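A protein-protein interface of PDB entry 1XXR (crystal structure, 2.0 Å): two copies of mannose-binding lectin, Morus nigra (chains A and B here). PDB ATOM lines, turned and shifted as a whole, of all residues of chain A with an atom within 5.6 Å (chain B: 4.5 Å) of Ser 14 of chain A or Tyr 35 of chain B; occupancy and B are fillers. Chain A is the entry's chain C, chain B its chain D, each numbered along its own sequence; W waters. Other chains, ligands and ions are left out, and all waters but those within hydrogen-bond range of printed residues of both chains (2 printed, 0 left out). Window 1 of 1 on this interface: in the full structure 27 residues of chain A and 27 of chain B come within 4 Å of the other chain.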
ATOM      1  N   GLY A  12     -13.401  29.084  25.637  1.00  0.00           N
ATOM      2  CA  GLY A  12     -13.936  28.511  24.413  1.00  0.00           C
ATOM      3  C   GLY A  12     -14.755  27.249  24.599  1.00  0.00           C
ATOM      4  O   GLY A  12     -15.211  26.655  23.625  1.00  0.00           O
ATOM      5  N   THR A  13     -14.948  26.836  25.847  1.00  0.00           N
ATOM      6  CA  THR A  13     -15.722  25.634  26.143  1.00  0.00           C
ATOM      7  C   THR A  13     -17.142  25.999  26.572  1.00  0.00           C
ATOM      8  O   THR A  13     -17.326  26.713  27.555  1.00  0.00           O
ATOM      9  CB  THR A  13     -15.056  24.825  27.278  1.00  0.00           C
ATOM     10  OG1 THR A  13     -13.738  24.436  26.873  1.00  0.00           O
ATOM     11  CG2 THR A  13     -15.872  23.582  27.603  1.00  0.00           C
ATOM     12  N   SER A  14     -18.140  25.518  25.834  1.00  0.00           N
ATOM     13  CA  SER A  14     -19.532  25.804  26.172  1.00  0.00           C
ATOM     14  C   SER A  14     -19.907  25.010  27.417  1.00  0.00           C
ATOM     15  O   SER A  14     -19.144  24.157  27.876  1.00  0.00           O
ATOM     16  CB  SER A  14     -20.471  25.433  25.013  1.00  0.00           C
ATOM     17  OG  SER A  14     -20.440  24.041  24.737  1.00  0.00           O
ATOM     18  N   GLN A  15     -21.084  25.272  27.966  1.00  0.00           N
ATOM     19  CA  GLN A  15     -21.475  24.560  29.172  1.00  0.00           C
ATOM     20  C   GLN A  15     -22.957  24.217  29.216  1.00  0.00           C
ATOM     21  O   GLN A  15     -23.739  24.666  28.379  1.00  0.00           O
ATOM     22  CB  GLN A  15     -21.100  25.401  30.396  1.00  0.00           C
ATOM     23  CG  GLN A  15     -21.892  26.680  30.528  1.00  0.00           C
ATOM     24  CD  GLN A  15     -21.351  27.609  31.603  1.00  0.00           C
ATOM     25  OE1 GLN A  15     -21.014  27.176  32.709  1.00  0.00           O
ATOM     26  NE2 GLN A  15     -21.282  28.901  31.286  1.00  0.00           N
ATOM     27  N   THR A  16     -23.321  23.388  30.190  1.00  0.00           N
ATOM     28  CA  THR A  16     -24.708  23.005  30.393  1.00  0.00           C
ATOM     29  C   THR A  16     -24.960  23.010  31.890  1.00  0.00           C
ATOM     30  O   THR A  16     -24.027  23.021  32.699  1.00  0.00           O
ATOM     31  CB  THR A  16     -25.026  21.576  29.872  1.00  0.00           C
ATOM     32  OG1 THR A  16     -24.132  20.637  30.480  1.00  0.00           O
ATOM     33  CG2 THR A  16     -24.899  21.505  28.354  1.00  0.00           C
ATOM     34  N   LEU A  58     -25.848  12.399  18.873  1.00  0.00           N
ATOM     35  CA  LEU A  58     -25.001  13.552  18.639  1.00  0.00           C
ATOM     36  C   LEU A  58     -25.404  14.093  17.285  1.00  0.00           C
ATOM     37  O   LEU A  58     -24.895  13.656  16.246  1.00  0.00           O
ATOM     38  CB  LEU A  58     -23.517  13.186  18.632  1.00  0.00           C
ATOM     39  CG  LEU A  58     -22.580  14.368  18.334  1.00  0.00           C
ATOM     40  CD1 LEU A  58     -22.713  15.434  19.421  1.00  0.00           C
ATOM     41  CD2 LEU A  58     -21.142  13.882  18.257  1.00  0.00           C
ATOM     42  N   ASN A  59     -26.366  15.008  17.309  1.00  0.00           N
ATOM     43  CA  ASN A  59     -26.856  15.649  16.103  1.00  0.00           C
ATOM     44  C   ASN A  59     -27.426  14.685  15.062  1.00  0.00           C
ATOM     45  O   ASN A  59     -27.124  14.795  13.873  1.00  0.00           O
ATOM     46  CB  ASN A  59     -25.730  16.490  15.498  1.00  0.00           C
ATOM     47  CG  ASN A  59     -25.204  17.533  16.471  1.00  0.00           C
ATOM     48  OD1 ASN A  59     -24.001  17.594  16.758  1.00  0.00           O
ATOM     49  ND2 ASN A  59     -26.108  18.362  16.991  1.00  0.00           N
ATOM     50  N   ASP B  32     -24.359  21.119  10.822  1.00  0.00           N
ATOM     51  CA  ASP B  32     -23.435  20.275  11.575  1.00  0.00           C
ATOM     52  C   ASP B  32     -24.012  19.928  12.943  1.00  0.00           C
ATOM     53  O   ASP B  32     -23.611  18.943  13.561  1.00  0.00           O
ATOM     54  CB  ASP B  32     -22.085  20.979  11.798  1.00  0.00           C
ATOM     55  CG  ASP B  32     -21.287  21.166  10.519  1.00  0.00           C
ATOM     56  OD1 ASP B  32     -21.652  20.585   9.470  1.00  0.00           O
ATOM     57  OD2 ASP B  32     -20.272  21.896  10.575  1.00  0.00           O
ATOM     58  N   GLY B  33     -24.954  20.738  13.414  1.00  0.00           N
ATOM     59  CA  GLY B  33     -25.514  20.501  14.730  1.00  0.00           C
ATOM     60  C   GLY B  33     -24.658  21.277  15.718  1.00  0.00           C
ATOM     61  O   GLY B  33     -23.913  22.173  15.311  1.00  0.00           O
ATOM     62  N   SER B  34     -24.723  20.933  17.000  1.00  0.00           N
ATOM     63  CA  SER B  34     -23.948  21.656  18.006  1.00  0.00           C
ATOM     64  C   SER B  34     -22.949  20.788  18.766  1.00  0.00           C
ATOM     65  O   SER B  34     -23.124  19.578  18.886  1.00  0.00           O
ATOM     66  CB  SER B  34     -24.896  22.331  19.002  1.00  0.00           C
ATOM     67  OG  SER B  34     -25.681  21.359  19.662  1.00  0.00           O
ATOM     68  N   TYR B  35     -21.903  21.426  19.283  1.00  0.00           N
ATOM     69  CA  TYR B  35     -20.852  20.728  20.020  1.00  0.00           C
ATOM     70  C   TYR B  35     -20.421  21.535  21.250  1.00  0.00           C
ATOM     71  O   TYR B  35     -21.180  22.368  21.749  1.00  0.00           O
ATOM     72  CB  TYR B  35     -19.654  20.474  19.086  1.00  0.00           C
ATOM     73  CG  TYR B  35     -20.044  19.773  17.799  1.00  0.00           C
ATOM     74  CD1 TYR B  35     -20.680  20.469  16.764  1.00  0.00           C
ATOM     75  CD2 TYR B  35     -19.841  18.403  17.640  1.00  0.00           C
ATOM     76  CE1 TYR B  35     -21.108  19.813  15.605  1.00  0.00           C
ATOM     77  CE2 TYR B  35     -20.268  17.737  16.481  1.00  0.00           C
ATOM     78  CZ  TYR B  35     -20.899  18.447  15.470  1.00  0.00           C
ATOM     79  OH  TYR B  35     -21.315  17.792  14.327  1.00  0.00           O
ATOM     80  N   THR B  36     -19.206  21.290  21.736  1.00  0.00           N
ATOM     81  CA  THR B  36     -18.694  21.991  22.913  1.00  0.00           C
ATOM     82  C   THR B  36     -17.858  23.217  22.550  1.00  0.00           C
ATOM     83  O   THR B  36     -17.657  24.111  23.375  1.00  0.00           O
ATOM     84  CB  THR B  36     -17.826  21.046  23.782  1.00  0.00           C
ATOM     85  OG1 THR B  36     -18.621  19.943  24.220  1.00  0.00           O
ATOM     86  CG2 THR B  36     -17.294  21.775  25.006  1.00  0.00           C
ATOM     87  N   GLY B  37     -17.367  23.257  21.316  1.00  0.00           N
ATOM     88  CA  GLY B  37     -16.559  24.383  20.887  1.00  0.00           C
ATOM     89  C   GLY B  37     -15.942  24.165  19.519  1.00  0.00           C
ATOM     90  O   GLY B  37     -16.259  23.191  18.835  1.00  0.00           O
ATOM     91  N   TYR B  56     -14.607  20.259  15.498  1.00  0.00           N
ATOM     92  CA  TYR B  56     -15.186  20.798  16.719  1.00  0.00           C
ATOM     93  C   TYR B  56     -14.559  20.177  17.939  1.00  0.00           C
ATOM     94  O   TYR B  56     -13.779  19.231  17.841  1.00  0.00           O
ATOM     95  CB  TYR B  56     -16.686  20.495  16.777  1.00  0.00           C
ATOM     96  CG  TYR B  56     -17.499  21.137  15.689  1.00  0.00           C
ATOM     97  CD1 TYR B  56     -17.863  20.428  14.541  1.00  0.00           C
ATOM     98  CD2 TYR B  56     -17.923  22.456  15.814  1.00  0.00           C
ATOM     99  CE1 TYR B  56     -18.640  21.034  13.543  1.00  0.00           C
ATOM    100  CE2 TYR B  56     -18.689  23.063  14.836  1.00  0.00           C
ATOM    101  CZ  TYR B  56     -19.047  22.351  13.706  1.00  0.00           C
ATOM    102  OH  TYR B  56     -19.830  22.973  12.765  1.00  0.00           O
ATOM    103  N   ASP B  57     -14.889  20.732  19.097  1.00  0.00           N
ATOM    104  CA  ASP B  57     -14.434  20.132  20.332  1.00  0.00           C
ATOM    105  C   ASP B  57     -15.690  19.446  20.837  1.00  0.00           C
ATOM    106  O   ASP B  57     -16.787  19.999  20.737  1.00  0.00           O
ATOM    107  CB  ASP B  57     -14.005  21.146  21.381  1.00  0.00           C
ATOM    108  CG  ASP B  57     -13.656  20.474  22.701  1.00  0.00           C
ATOM    109  OD1 ASP B  57     -12.641  19.745  22.738  1.00  0.00           O
ATOM    110  OD2 ASP B  57     -14.405  20.650  23.692  1.00  0.00           O
ATOM    111  N   PHE B  63     -13.559  16.451  17.347  1.00  0.00           N
ATOM    112  CA  PHE B  63     -14.568  15.677  16.633  1.00  0.00           C
ATOM    113  C   PHE B  63     -14.646  16.271  15.235  1.00  0.00           C
ATOM    114  O   PHE B  63     -14.937  17.459  15.073  1.00  0.00           O
ATOM    115  CB  PHE B  63     -15.940  15.784  17.309  1.00  0.00           C
ATOM    116  CG  PHE B  63     -17.014  14.975  16.627  1.00  0.00           C
ATOM    117  CD1 PHE B  63     -17.185  13.624  16.925  1.00  0.00           C
ATOM    118  CD2 PHE B  63     -17.820  15.551  15.651  1.00  0.00           C
ATOM    119  CE1 PHE B  63     -18.148  12.857  16.256  1.00  0.00           C
ATOM    120  CE2 PHE B  63     -18.784  14.795  14.976  1.00  0.00           C
ATOM    121  CZ  PHE B  63     -18.948  13.445  15.279  1.00  0.00           C
ATOM    122  N   PRO B  66     -19.087  17.172   9.713  1.00  0.00           N
ATOM    123  CA  PRO B  66     -19.408  16.817   8.330  1.00  0.00           C
ATOM    124  C   PRO B  66     -18.651  17.747   7.382  1.00  0.00           C
ATOM    125  O   PRO B  66     -18.481  18.931   7.671  1.00  0.00           O
ATOM    126  CB  PRO B  66     -20.915  17.041   8.264  1.00  0.00           C
ATOM    127  CG  PRO B  66     -21.359  16.697   9.653  1.00  0.00           C
ATOM    128  CD  PRO B  66     -20.314  17.375  10.504  1.00  0.00           C
ATOM    129  N   LEU B 140     -20.979  31.453  22.874  1.00  0.00           N
ATOM    130  CA  LEU B 140     -20.059  30.920  21.878  1.00  0.00           C
ATOM    131  C   LEU B 140     -20.752  30.293  20.677  1.00  0.00           C
ATOM    132  O   LEU B 140     -21.892  29.833  20.765  1.00  0.00           O
ATOM    133  CB  LEU B 140     -19.193  29.828  22.514  1.00  0.00           C
ATOM    134  CG  LEU B 140     -18.228  30.157  23.650  1.00  0.00           C
ATOM    135  CD1 LEU B 140     -17.940  28.898  24.463  1.00  0.00           C
ATOM    136  CD2 LEU B 140     -16.954  30.745  23.073  1.00  0.00           C
ATOM    137  N   VAL B 142     -21.154  27.257  18.688  1.00  0.00           N
ATOM    138  CA  VAL B 142     -20.876  25.852  18.972  1.00  0.00           C
ATOM    139  C   VAL B 142     -21.251  24.940  17.815  1.00  0.00           C
ATOM    140  O   VAL B 142     -21.229  23.713  17.947  1.00  0.00           O
ATOM    141  CB  VAL B 142     -21.628  25.377  20.235  1.00  0.00           C
ATOM    142  CG1 VAL B 142     -21.048  26.055  21.473  1.00  0.00           C
ATOM    143  CG2 VAL B 142     -23.117  25.696  20.106  1.00  0.00           C
ATOM    144  N   SER B 160     -24.416  29.144  22.215  1.00  0.00           N
ATOM    145  CA  SER B 160     -24.640  28.569  23.531  1.00  0.00           C
ATOM    146  C   SER B 160     -23.761  29.227  24.587  1.00  0.00           C
ATOM    147  O   SER B 160     -22.689  29.748  24.276  1.00  0.00           O
ATOM    148  CB  SER B 160     -24.335  27.066  23.501  1.00  0.00           C
ATOM    149  OG  SER B 160     -24.308  26.530  24.812  1.00  0.00           O
ATOM    150  N   LEU B 161     -24.226  29.209  25.835  1.00  0.00           N
ATOM    151  CA  LEU B 161     -23.442  29.751  26.941  1.00  0.00           C
ATOM    152  C   LEU B 161     -22.408  28.687  27.319  1.00  0.00           C
ATOM    153  O   LEU B 161     -21.479  29.001  28.093  1.00  0.00           O
ATOM    154  CB  LEU B 161     -24.325  30.052  28.160  1.00  0.00           C
ATOM    155  CG  LEU B 161     -25.231  31.293  28.170  1.00  0.00           C
ATOM    156  CD1 LEU B 161     -24.433  32.519  27.727  1.00  0.00           C
ATOM    157  CD2 LEU B 161     -26.412  31.078  27.253  1.00  0.00           C
ATOM    158  OXT LEU B 161     -22.549  27.538  26.839  1.00  0.00           O
HETATM  159  O   HOH W   1     -18.869  28.923  28.150  1.00  0.00           O
HETATM  160  O   HOH W   2     -13.603  21.289  26.057  1.00  0.00           O
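Among the printed residues, merely in contact across the chains: Asn 59 of chain A with Gly 33 of chain B, Asn 59 of chain A with Tyr 35 of chain B, Thr 13 of chain A with Thr 36 of chain B, Ser 14 of chain A with Leu 161 of chain B, Ser 14 of chain A with Tyr 35 of chain B, Gly 12 of chain A with Thr 36 of chain B, Gly 12 of chain A with Leu 140 of chain B, Ser 14 of chain A with Val 142 of chain B, Ser 14 of chain A with Leu 140 of chain B, Thr 13 of chain A with Leu 140 of chain B, Leu 58 of chain A with Phe 63 of chain B, Gly 12 of chain A with Gly 37 of chain B and Ser 14 of chain A with Ser 160 of chain B.
Hydrophobic or aromatic side chains of chain A within 4 Å of the printed part of chain B: Leu 58.
Hydrophobic or aromatic side chains of chain B that line the printed part of chain A: Tyr 35, Phe 63, Leu 140 and Val 142.
Among the printed residues, 17 pairs touch across the chains.
Among the printed residues, no Asp or Glu carboxylate lies within 4 Å of a Lys or Arg side-chain nitrogen of the other chain.
No position is printed for both chains.
N of Asp 57 of chain B lies within hydrogen-bond range of O of Gly 37 of chain B, 2.8 Å away.
O of Asp 32 of chain B sits at hydrogen-bond distance from OH of Tyr 35 of chain B, 2.7 Å away.
The backbone NH (N) of Phe 63 of chain B lies within hydrogen-bond range of the backbone carbonyl oxygen (O) of Tyr 56 of chain B, 2.8 Å away.
The backbone NH (N) of Leu 140 of chain B lies within hydrogen-bond range of the backbone carbonyl oxygen (O) of Ser 160 of chain B (2.8 Å).
O of Val 142 of chain B lies within hydrogen-bond range of N of Tyr 35 of chain B, at 2.7 Å.
OD2 of Asp 32 of chain B sits at hydrogen-bond distance from OH of Tyr 56 of chain B, at 2.5 Å.
The backbone NH (N) of Ser 34 of chain B sits close to the side-chain amide nitrogen (ND2) of Asn 59 of chain A, at 2.9 Å.
The backbone NH (N) of Gln 15 of chain A sits at hydrogen-bond distance from the chain-end carboxylate (OXT) of Leu 161 of chain B, at 2.9 Å.
OD1 of Asn 59 of chain A lies close to O of Asp 32 of chain B.
O of Thr 36 of chain B is in hydrogen-bond range of N of Ser 14 of chain A, 2.9 Å away.
Water W2 bridges OD2 of Asp 57 of chain B (2.6 Å) and OG1 of Thr 13 of chain A (3.3 Å).
Water W1 bridges O of Leu 161 of chain B (2.6 Å) and O of Thr 13 of chain A (2.8 Å).
Printed residues of chain B within 4 Å of Ser 14 of chain A: Tyr 35 (3.5 Å), Thr 36 (2.9 Å), Leu 140 (3.7 Å), Val 142 (3.6 Å), Ser 160 (3.996 Å) and Leu 161 (3.5 Å).
Printed residues of chain A within 4 Å of Tyr 35 of chain B: Ser 14 and Asn 59.
Of the printed residues of chain B, Gln 15 of chain A touches Leu 161 (2.9 Å).
Of the printed residues of chain A, Leu 161 of chain B touches Ser 14 (3.5 Å) and Gln 15 (2.9 Å).
Of the printed residues of chain B, Thr 13 of chain A touches Thr 36 and Leu 140.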
